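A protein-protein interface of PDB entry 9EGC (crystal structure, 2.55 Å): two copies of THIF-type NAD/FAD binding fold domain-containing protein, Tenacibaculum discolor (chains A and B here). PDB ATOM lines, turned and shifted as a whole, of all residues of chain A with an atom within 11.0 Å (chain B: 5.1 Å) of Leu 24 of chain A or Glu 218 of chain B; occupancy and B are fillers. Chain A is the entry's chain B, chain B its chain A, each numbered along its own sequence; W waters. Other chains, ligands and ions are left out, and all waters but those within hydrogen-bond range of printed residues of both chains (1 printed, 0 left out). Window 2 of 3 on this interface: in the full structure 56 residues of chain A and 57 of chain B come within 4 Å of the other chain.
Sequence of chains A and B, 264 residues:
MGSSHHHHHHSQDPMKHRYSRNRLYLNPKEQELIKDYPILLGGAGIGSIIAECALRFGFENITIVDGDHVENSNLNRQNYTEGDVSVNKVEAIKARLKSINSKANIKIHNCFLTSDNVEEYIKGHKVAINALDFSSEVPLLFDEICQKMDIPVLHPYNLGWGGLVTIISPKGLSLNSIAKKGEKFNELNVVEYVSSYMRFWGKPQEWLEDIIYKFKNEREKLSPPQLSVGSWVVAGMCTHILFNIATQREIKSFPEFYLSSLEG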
ATOM      1  N   MET A  15      -8.463   9.729  12.171  1.00  0.00           N
ATOM      2  CA  MET A  15      -8.143  10.361  13.447  1.00  0.00           C
ATOM      3  C   MET A  15      -7.462  11.741  13.265  1.00  0.00           C
ATOM      4  O   MET A  15      -7.251  12.217  12.140  1.00  0.00           O
ATOM      5  CB  MET A  15      -7.255   9.421  14.297  1.00  0.00           C
ATOM      6  CG  MET A  15      -7.961   8.117  14.759  1.00  0.00           C
ATOM      7  SD  MET A  15      -7.053   6.930  15.814  1.00  0.00           S
ATOM      8  CE  MET A  15      -8.423   6.204  16.693  1.00  0.00           C
ATOM      9  N   TYR A  19      -7.253  13.057  18.815  1.00  0.00           N
ATOM     10  CA  TYR A  19      -7.673  11.695  19.134  1.00  0.00           C
ATOM     11  C   TYR A  19      -6.507  10.713  19.103  1.00  0.00           C
ATOM     12  O   TYR A  19      -6.714   9.504  18.942  1.00  0.00           O
ATOM     13  CB  TYR A  19      -8.788  11.225  18.192  1.00  0.00           C
ATOM     14  CG  TYR A  19     -10.013  12.112  18.218  1.00  0.00           C
ATOM     15  CD1 TYR A  19     -10.722  12.301  19.400  1.00  0.00           C
ATOM     16  CD2 TYR A  19     -10.455  12.760  17.069  1.00  0.00           C
ATOM     17  CE1 TYR A  19     -11.827  13.112  19.440  1.00  0.00           C
ATOM     18  CE2 TYR A  19     -11.559  13.583  17.101  1.00  0.00           C
ATOM     19  CZ  TYR A  19     -12.247  13.758  18.286  1.00  0.00           C
ATOM     20  OH  TYR A  19     -13.352  14.583  18.328  1.00  0.00           O
ATOM     21  N   SER A  20      -5.284  11.219  19.255  1.00  0.00           N
ATOM     22  CA  SER A  20      -4.099  10.374  19.198  1.00  0.00           C
ATOM     23  C   SER A  20      -4.171   9.242  20.225  1.00  0.00           C
ATOM     24  O   SER A  20      -3.896   8.076  19.910  1.00  0.00           O
ATOM     25  CB  SER A  20      -2.866  11.249  19.403  1.00  0.00           C
ATOM     26  OG  SER A  20      -1.740  10.469  19.704  1.00  0.00           O
ATOM     27  N   ARG A  21      -4.556   9.559  21.454  1.00  0.00           N
ATOM     28  CA  ARG A  21      -4.567   8.543  22.498  1.00  0.00           C
ATOM     29  C   ARG A  21      -5.774   7.606  22.416  1.00  0.00           C
ATOM     30  O   ARG A  21      -5.922   6.727  23.277  1.00  0.00           O
ATOM     31  CB  ARG A  21      -4.481   9.229  23.864  1.00  0.00           C
ATOM     32  CG  ARG A  21      -3.225  10.066  23.982  1.00  0.00           C
ATOM     33  CD  ARG A  21      -1.998   9.154  23.930  1.00  0.00           C
ATOM     34  NE  ARG A  21      -1.732   8.537  25.227  1.00  0.00           N
ATOM     35  CZ  ARG A  21      -0.902   9.050  26.128  1.00  0.00           C
ATOM     36  NH1 ARG A  21      -0.245  10.170  25.854  1.00  0.00           N
ATOM     37  NH2 ARG A  21      -0.724   8.442  27.295  1.00  0.00           N
ATOM     38  N   ASN A  22      -6.620   7.747  21.391  1.00  0.00           N
ATOM     39  CA  ASN A  22      -7.730   6.827  21.179  1.00  0.00           C
ATOM     40  C   ASN A  22      -7.324   5.536  20.486  1.00  0.00           C
ATOM     41  O   ASN A  22      -8.155   4.621  20.393  1.00  0.00           O
ATOM     42  CB  ASN A  22      -8.803   7.510  20.330  1.00  0.00           C
ATOM     43  CG  ASN A  22      -9.846   8.205  21.159  1.00  0.00           C
ATOM     44  OD1 ASN A  22      -9.691   8.362  22.378  1.00  0.00           O
ATOM     45  ND2 ASN A  22     -10.896   8.684  20.497  1.00  0.00           N
ATOM     46  N   ARG A  23      -6.079   5.429  20.027  1.00  0.00           N
ATOM     47  CA  ARG A  23      -5.676   4.321  19.173  1.00  0.00           C
ATOM     48  C   ARG A  23      -5.747   2.986  19.920  1.00  0.00           C
ATOM     49  O   ARG A  23      -5.826   2.928  21.154  1.00  0.00           O
ATOM     50  CB  ARG A  23      -4.269   4.562  18.643  1.00  0.00           C
ATOM     51  CG  ARG A  23      -3.237   4.577  19.745  1.00  0.00           C
ATOM     52  CD  ARG A  23      -1.821   4.668  19.203  1.00  0.00           C
ATOM     53  NE  ARG A  23      -0.882   3.930  20.033  1.00  0.00           N
ATOM     54  CZ  ARG A  23      -0.448   4.351  21.214  1.00  0.00           C
ATOM     55  NH1 ARG A  23      -0.874   5.515  21.703  1.00  0.00           N
ATOM     56  NH2 ARG A  23       0.412   3.610  21.904  1.00  0.00           N
ATOM     57  N   LEU A  24      -5.711   1.902  19.139  1.00  0.00           N
ATOM     58  CA  LEU A  24      -5.888   0.531  19.613  1.00  0.00           C
ATOM     59  C   LEU A  24      -7.324   0.288  20.070  1.00  0.00           C
ATOM     60  O   LEU A  24      -7.932  -0.702  19.657  1.00  0.00           O
ATOM     61  CB  LEU A  24      -4.907   0.193  20.740  1.00  0.00           C
ATOM     62  CG  LEU A  24      -3.401   0.312  20.484  1.00  0.00           C
ATOM     63  CD1 LEU A  24      -2.632  -0.260  21.674  1.00  0.00           C
ATOM     64  CD2 LEU A  24      -2.976  -0.341  19.164  1.00  0.00           C
ATOM     65  N   TYR A  25      -7.863   1.153  20.944  1.00  0.00           N
ATOM     66  CA  TYR A  25      -9.280   1.070  21.306  1.00  0.00           C
ATOM     67  C   TYR A  25     -10.181   1.340  20.105  1.00  0.00           C
ATOM     68  O   TYR A  25     -11.191   0.652  19.907  1.00  0.00           O
ATOM     69  CB  TYR A  25      -9.611   2.059  22.418  1.00  0.00           C
ATOM     70  CG  TYR A  25      -9.025   1.729  23.758  1.00  0.00           C
ATOM     71  CD1 TYR A  25      -9.450   0.612  24.463  1.00  0.00           C
ATOM     72  CD2 TYR A  25      -8.072   2.554  24.346  1.00  0.00           C
ATOM     73  CE1 TYR A  25      -8.922   0.309  25.710  1.00  0.00           C
ATOM     74  CE2 TYR A  25      -7.540   2.260  25.596  1.00  0.00           C
ATOM     75  CZ  TYR A  25      -7.968   1.136  26.272  1.00  0.00           C
ATOM     76  OH  TYR A  25      -7.449   0.839  27.509  1.00  0.00           O
ATOM     77  N   LEU A  26      -9.851   2.350  19.308  1.00  0.00           N
ATOM     78  CA  LEU A  26     -10.596   2.662  18.098  1.00  0.00           C
ATOM     79  C   LEU A  26      -9.640   2.633  16.916  1.00  0.00           C
ATOM     80  O   LEU A  26      -8.510   3.122  17.011  1.00  0.00           O
ATOM     81  CB  LEU A  26     -11.263   4.045  18.159  1.00  0.00           C
ATOM     82  CG  LEU A  26     -12.488   4.308  19.037  1.00  0.00           C
ATOM     83  CD1 LEU A  26     -12.103   4.417  20.511  1.00  0.00           C
ATOM     84  CD2 LEU A  26     -13.230   5.549  18.553  1.00  0.00           C
ATOM     85  N   ASN A  27     -10.078   2.045  15.824  1.00  0.00           N
ATOM     86  CA  ASN A  27      -9.281   2.194  14.620  1.00  0.00           C
ATOM     87  C   ASN A  27      -9.727   3.443  13.864  1.00  0.00           C
ATOM     88  O   ASN A  27     -10.801   3.990  14.138  1.00  0.00           O
ATOM     89  CB  ASN A  27      -9.396   0.936  13.762  1.00  0.00           C
ATOM     90  CG  ASN A  27     -10.805   0.675  13.288  1.00  0.00           C
ATOM     91  OD1 ASN A  27     -11.367   1.443  12.508  1.00  0.00           O
ATOM     92  ND2 ASN A  27     -11.386  -0.420  13.760  1.00  0.00           N
ATOM     93  N   PRO A  28      -8.928   3.934  12.912  1.00  0.00           N
ATOM     94  CA  PRO A  28      -9.294   5.196  12.231  1.00  0.00           C
ATOM     95  C   PRO A  28     -10.683   5.213  11.599  1.00  0.00           C
ATOM     96  O   PRO A  28     -11.341   6.266  11.602  1.00  0.00           O
ATOM     97  CB  PRO A  28      -8.181   5.368  11.182  1.00  0.00           C
ATOM     98  CG  PRO A  28      -7.375   4.096  11.208  1.00  0.00           C
ATOM     99  CD  PRO A  28      -7.562   3.507  12.566  1.00  0.00           C
ATOM    100  N   LYS A  29     -11.153   4.087  11.054  1.00  0.00           N
ATOM    101  CA  LYS A  29     -12.470   4.078  10.419  1.00  0.00           C
ATOM    102  C   LYS A  29     -13.590   4.231  11.444  1.00  0.00           C
ATOM    103  O   LYS A  29     -14.638   4.809  11.132  1.00  0.00           O
ATOM    104  CB  LYS A  29     -12.646   2.806   9.586  1.00  0.00           C
ATOM    105  CG  LYS A  29     -11.809   2.824   8.310  1.00  0.00           C
ATOM    106  CD  LYS A  29     -12.204   1.748   7.319  1.00  0.00           C
ATOM    107  CE  LYS A  29     -11.521   1.976   5.971  1.00  0.00           C
ATOM    108  NZ  LYS A  29     -10.028   1.947   6.044  1.00  0.00           N
ATOM    109  N   GLU A  30     -13.396   3.720  12.661  1.00  0.00           N
ATOM    110  CA  GLU A  30     -14.386   3.930  13.709  1.00  0.00           C
ATOM    111  C   GLU A  30     -14.392   5.384  14.166  1.00  0.00           C
ATOM    112  O   GLU A  30     -15.460   5.971  14.384  1.00  0.00           O
ATOM    113  CB  GLU A  30     -14.099   3.005  14.889  1.00  0.00           C
ATOM    114  CG  GLU A  30     -14.004   1.546  14.500  1.00  0.00           C
ATOM    115  CD  GLU A  30     -13.642   0.646  15.664  1.00  0.00           C
ATOM    116  OE1 GLU A  30     -14.372  -0.337  15.910  1.00  0.00           O
ATOM    117  OE2 GLU A  30     -12.622   0.916  16.331  1.00  0.00           O
ATOM    118  N   GLN A  31     -13.200   5.974  14.313  1.00  0.00           N
ATOM    119  CA  GLN A  31     -13.087   7.375  14.708  1.00  0.00           C
ATOM    120  C   GLN A  31     -13.803   8.286  13.720  1.00  0.00           C
ATOM    121  O   GLN A  31     -14.486   9.238  14.121  1.00  0.00           O
ATOM    122  CB  GLN A  31     -11.605   7.759  14.828  1.00  0.00           C
ATOM    123  CG  GLN A  31     -11.331   9.076  15.566  1.00  0.00           C
ATOM    124  CD  GLN A  31     -11.583   8.973  17.066  1.00  0.00           C
ATOM    125  OE1 GLN A  31     -10.889   8.230  17.773  1.00  0.00           O
ATOM    126  NE2 GLN A  31     -12.598   9.698  17.557  1.00  0.00           N
ATOM    127  N   PHE A  57     -14.449  11.954  23.287  1.00  0.00           N
ATOM    128  CA  PHE A  57     -14.274  10.632  22.694  1.00  0.00           C
ATOM    129  C   PHE A  57     -14.228  10.696  21.166  1.00  0.00           C
ATOM    130  O   PHE A  57     -13.534   9.897  20.531  1.00  0.00           O
ATOM    131  CB  PHE A  57     -15.417   9.737  23.173  1.00  0.00           C
ATOM    132  CG  PHE A  57     -15.283   8.286  22.798  1.00  0.00           C
ATOM    133  CD1 PHE A  57     -14.555   7.418  23.599  1.00  0.00           C
ATOM    134  CD2 PHE A  57     -15.924   7.776  21.684  1.00  0.00           C
ATOM    135  CE1 PHE A  57     -14.438   6.067  23.277  1.00  0.00           C
ATOM    136  CE2 PHE A  57     -15.810   6.432  21.355  1.00  0.00           C
ATOM    137  CZ  PHE A  57     -15.063   5.577  22.156  1.00  0.00           C
ATOM    138  N   PHE A 243     -20.662   4.284  21.563  1.00  0.00           N
ATOM    139  CA  PHE A 243     -19.667   3.677  20.691  1.00  0.00           C
ATOM    140  C   PHE A 243     -20.109   2.288  20.236  1.00  0.00           C
ATOM    141  O   PHE A 243     -19.892   1.910  19.080  1.00  0.00           O
ATOM    142  CB  PHE A 243     -18.322   3.606  21.409  1.00  0.00           C
ATOM    143  CG  PHE A 243     -17.267   2.898  20.626  1.00  0.00           C
ATOM    144  CD1 PHE A 243     -16.678   3.511  19.524  1.00  0.00           C
ATOM    145  CD2 PHE A 243     -16.865   1.615  20.978  1.00  0.00           C
ATOM    146  CE1 PHE A 243     -15.705   2.849  18.783  1.00  0.00           C
ATOM    147  CE2 PHE A 243     -15.890   0.949  20.250  1.00  0.00           C
ATOM    148  CZ  PHE A 243     -15.310   1.564  19.149  1.00  0.00           C
ATOM    149  N   THR A 247     -20.971   1.353  16.231  1.00  0.00           N
ATOM    150  CA  THR A 247     -20.134   0.314  15.647  1.00  0.00           C
ATOM    151  C   THR A 247     -20.809  -1.049  15.613  1.00  0.00           C
ATOM    152  O   THR A 247     -20.156  -2.044  15.276  1.00  0.00           O
ATOM    153  CB  THR A 247     -18.831   0.199  16.432  1.00  0.00           C
ATOM    154  OG1 THR A 247     -19.128  -0.176  17.792  1.00  0.00           O
ATOM    155  CG2 THR A 247     -18.085   1.542  16.413  1.00  0.00           C
ATOM    156  N   ARG A 249     -21.789  -3.123  17.900  1.00  0.00           N
ATOM    157  CA  ARG A 249     -21.420  -4.106  18.906  1.00  0.00           C
ATOM    158  C   ARG A 249     -22.628  -4.357  19.795  1.00  0.00           C
ATOM    159  O   ARG A 249     -23.463  -3.472  19.983  1.00  0.00           O
ATOM    160  CB  ARG A 249     -20.237  -3.606  19.740  1.00  0.00           C
ATOM    161  CG  ARG A 249     -18.902  -3.491  18.997  1.00  0.00           C
ATOM    162  CD  ARG A 249     -17.869  -2.808  19.877  1.00  0.00           C
ATOM    163  NE  ARG A 249     -16.484  -3.079  19.495  1.00  0.00           N
ATOM    164  CZ  ARG A 249     -15.780  -2.346  18.633  1.00  0.00           C
ATOM    165  NH1 ARG A 249     -16.331  -1.293  18.051  1.00  0.00           N
ATOM    166  NH2 ARG A 249     -14.519  -2.653  18.365  1.00  0.00           N
ATOM    167  N   ILE B 211      -6.434  -5.317  25.219  1.00  0.00           N
ATOM    168  CA  ILE B 211      -5.747  -4.043  25.022  1.00  0.00           C
ATOM    169  C   ILE B 211      -4.304  -4.105  25.526  1.00  0.00           C
ATOM    170  O   ILE B 211      -3.414  -3.468  24.948  1.00  0.00           O
ATOM    171  CB  ILE B 211      -6.547  -2.894  25.665  1.00  0.00           C
ATOM    172  CG1 ILE B 211      -6.006  -1.552  25.185  1.00  0.00           C
ATOM    173  CG2 ILE B 211      -6.509  -2.971  27.176  1.00  0.00           C
ATOM    174  CD1 ILE B 211      -6.169  -1.335  23.701  1.00  0.00           C
ATOM    175  N   LYS B 214      -2.501  -5.914  22.567  1.00  0.00           N
ATOM    176  CA  LYS B 214      -2.334  -5.024  21.416  1.00  0.00           C
ATOM    177  C   LYS B 214      -1.213  -4.021  21.651  1.00  0.00           C
ATOM    178  O   LYS B 214      -0.408  -3.753  20.750  1.00  0.00           O
ATOM    179  CB  LYS B 214      -3.635  -4.267  21.119  1.00  0.00           C
ATOM    180  CG  LYS B 214      -4.789  -5.087  20.585  1.00  0.00           C
ATOM    181  CD  LYS B 214      -5.917  -4.170  20.120  1.00  0.00           C
ATOM    182  CE  LYS B 214      -7.219  -4.926  19.855  1.00  0.00           C
ATOM    183  NZ  LYS B 214      -7.123  -5.880  18.716  1.00  0.00           N
ATOM    184  N   PHE B 215      -1.157  -3.449  22.858  1.00  0.00           N
ATOM    185  CA  PHE B 215      -0.177  -2.409  23.159  1.00  0.00           C
ATOM    186  C   PHE B 215       1.250  -2.951  23.157  1.00  0.00           C
ATOM    187  O   PHE B 215       2.157  -2.309  22.615  1.00  0.00           O
ATOM    188  CB  PHE B 215      -0.533  -1.738  24.490  1.00  0.00           C
ATOM    189  CG  PHE B 215       0.499  -0.751  24.975  1.00  0.00           C
ATOM    190  CD1 PHE B 215       0.881   0.326  24.188  1.00  0.00           C
ATOM    191  CD2 PHE B 215       1.051  -0.876  26.246  1.00  0.00           C
ATOM    192  CE1 PHE B 215       1.834   1.238  24.641  1.00  0.00           C
ATOM    193  CE2 PHE B 215       1.994   0.032  26.707  1.00  0.00           C
ATOM    194  CZ  PHE B 215       2.384   1.093  25.904  1.00  0.00           C
ATOM    195  N   LYS B 216       1.472  -4.134  23.735  1.00  0.00           N
ATOM    196  CA  LYS B 216       2.830  -4.675  23.776  1.00  0.00           C
ATOM    197  C   LYS B 216       3.352  -4.981  22.382  1.00  0.00           C
ATOM    198  O   LYS B 216       4.520  -4.718  22.080  1.00  0.00           O
ATOM    199  CB  LYS B 216       2.883  -5.933  24.634  1.00  0.00           C
ATOM    200  CG  LYS B 216       2.541  -5.706  26.080  1.00  0.00           C
ATOM    201  CD  LYS B 216       2.985  -6.890  26.909  1.00  0.00           C
ATOM    202  CE  LYS B 216       2.383  -6.810  28.283  1.00  0.00           C
ATOM    203  NZ  LYS B 216       2.788  -7.942  29.158  1.00  0.00           N
ATOM    204  N   ASN B 217       2.511  -5.542  21.520  1.00  0.00           N
ATOM    205  CA  ASN B 217       2.961  -5.898  20.184  1.00  0.00           C
ATOM    206  C   ASN B 217       2.957  -4.717  19.219  1.00  0.00           C
ATOM    207  O   ASN B 217       3.005  -4.919  18.002  1.00  0.00           O
ATOM    208  CB  ASN B 217       2.104  -7.034  19.631  1.00  0.00           C
ATOM    209  CG  ASN B 217       2.216  -8.298  20.462  1.00  0.00           C
ATOM    210  OD1 ASN B 217       3.310  -8.799  20.733  1.00  0.00           O
ATOM    211  ND2 ASN B 217       1.070  -8.836  20.854  1.00  0.00           N
ATOM    212  N   GLU B 218       2.870  -3.496  19.730  1.00  0.00           N
ATOM    213  CA  GLU B 218       3.058  -2.320  18.896  1.00  0.00           C
ATOM    214  C   GLU B 218       4.525  -2.164  18.515  1.00  0.00           C
ATOM    215  O   GLU B 218       5.412  -2.275  19.367  1.00  0.00           O
ATOM    216  CB  GLU B 218       2.564  -1.075  19.618  1.00  0.00           C
ATOM    217  CG  GLU B 218       1.308  -0.497  19.036  1.00  0.00           C
ATOM    218  CD  GLU B 218       0.965   0.815  19.679  1.00  0.00           C
ATOM    219  OE1 GLU B 218       1.472   1.071  20.793  1.00  0.00           O
ATOM    220  OE2 GLU B 218       0.219   1.604  19.060  1.00  0.00           O
ATOM    221  N   ARG B 219       4.769  -1.897  17.227  1.00  0.00           N
ATOM    222  CA  ARG B 219       6.125  -1.676  16.724  1.00  0.00           C
ATOM    223  C   ARG B 219       6.789  -0.493  17.420  1.00  0.00           C
ATOM    224  O   ARG B 219       7.819  -0.641  18.087  1.00  0.00           O
ATOM    225  CB  ARG B 219       6.060  -1.444  15.210  1.00  0.00           C
ATOM    226  CG  ARG B 219       7.366  -1.106  14.507  1.00  0.00           C
ATOM    227  CD  ARG B 219       8.376  -2.231  14.466  1.00  0.00           C
ATOM    228  NE  ARG B 219       9.571  -1.799  13.743  1.00  0.00           N
ATOM    229  CZ  ARG B 219      10.672  -2.529  13.620  1.00  0.00           C
ATOM    230  NH1 ARG B 219      10.727  -3.729  14.175  1.00  0.00           N
ATOM    231  NH2 ARG B 219      11.714  -2.059  12.941  1.00  0.00           N
ATOM    232  N   GLU B 220       6.197   0.687  17.287  1.00  0.00           N
ATOM    233  CA  GLU B 220       6.736   1.876  17.921  1.00  0.00           C
ATOM    234  C   GLU B 220       6.409   1.874  19.405  1.00  0.00           C
ATOM    235  O   GLU B 220       5.401   1.311  19.841  1.00  0.00           O
ATOM    236  CB  GLU B 220       6.174   3.131  17.261  1.00  0.00           C
ATOM    237  CG  GLU B 220       6.453   3.195  15.768  1.00  0.00           C
ATOM    238  CD  GLU B 220       5.977   4.488  15.148  1.00  0.00           C
ATOM    239  OE1 GLU B 220       4.819   4.887  15.404  1.00  0.00           O
ATOM    240  OE2 GLU B 220       6.769   5.100  14.395  1.00  0.00           O
ATOM    241  N   LEU B 222       5.105   3.960  22.241  1.00  0.00           N
ATOM    242  CA  LEU B 222       4.274   5.133  22.442  1.00  0.00           C
ATOM    243  C   LEU B 222       3.675   5.043  23.838  1.00  0.00           C
ATOM    244  O   LEU B 222       3.770   4.009  24.507  1.00  0.00           O
ATOM    245  CB  LEU B 222       3.172   5.201  21.379  1.00  0.00           C
ATOM    246  CG  LEU B 222       3.657   5.175  19.919  1.00  0.00           C
ATOM    247  CD1 LEU B 222       2.485   4.978  18.961  1.00  0.00           C
ATOM    248  CD2 LEU B 222       4.477   6.416  19.540  1.00  0.00           C
ATOM    249  N   PRO B 225      -2.676   4.058  25.234  1.00  0.00           N
ATOM    250  CA  PRO B 225      -3.905   4.769  24.886  1.00  0.00           C
ATOM    251  C   PRO B 225      -4.817   4.895  26.095  1.00  0.00           C
ATOM    252  O   PRO B 225      -4.760   4.096  27.030  1.00  0.00           O
ATOM    253  CB  PRO B 225      -4.522   3.888  23.797  1.00  0.00           C
ATOM    254  CG  PRO B 225      -3.979   2.534  24.061  1.00  0.00           C
ATOM    255  CD  PRO B 225      -2.594   2.741  24.581  1.00  0.00           C
HETATM  256  O   HOH W   1      -6.153   2.504  29.008  1.00  0.00           O
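OE2 of Glu 218 of chain B lies within salt-bridge range of NE of Arg 23 of chain A (2.8 Å).
Among the printed residues, pairs that only touch across the chains: Arg 23 of chain A with Pro 225 of chain B, Arg 21 of chain A with Pro 225 of chain B, Arg 23 of chain A with Leu 222 of chain B, Tyr 25 of chain A with Ile 211 of chain B, Leu 24 of chain A with Ile 211 of chain B, Leu 24 of chain A with Phe 215 of chain B, Tyr 25 of chain A with Pro 225 of chain B, Leu 24 of chain A with Glu 218 of chain B, Arg 23 of chain A with Phe 215 of chain B and Leu 24 of chain A with Pro 225 of chain B.
Printed residues of chain B within 4 Å of Leu 24 of chain A: Ile 211 (3.6 Å), Phe 215 (3.6 Å), Glu 218 (3.7 Å) and Pro 225 (3.9 Å).
Glu 218 of chain B touches two residues of chain A.
Of chain A, only Arg 23 and Leu 24 come within 4 Å of Phe 215 of chain B.
No residue of chain A comes within 4 Å of Asn 217 of chain B.
Of the printed residues of chain A, Ile 211 of chain B touches Leu 24 and Tyr 25.
Of the printed residues of chain A, Pro 225 of chain B touches Arg 21 (3.2 Å), Arg 23 (3.1 Å), Leu 24 (3.9 Å) and Tyr 25 (3.6 Å).
Of the printed residues of chain B, Arg 23 of chain A touches Phe 215, Glu 218, Leu 222 and Pro 225.
Printed residues of chain B within 4 Å of Arg 21 of chain A: Pro 225.
Lys 29 of chain A touches none of the printed residues of chain B.
Met 15 of chain A touches none of the printed residues of chain B.
Hydrophobic or aromatic side chains of chain A that line the printed part of chain B: Leu 24 and Tyr 25.
No position is printed for both chains.
Water W1 lies within hydrogen-bond range of the side-chain hydroxyl of Tyr 25 of chain A and the backbone carbonyl oxygen of Pro 225 of chain B.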
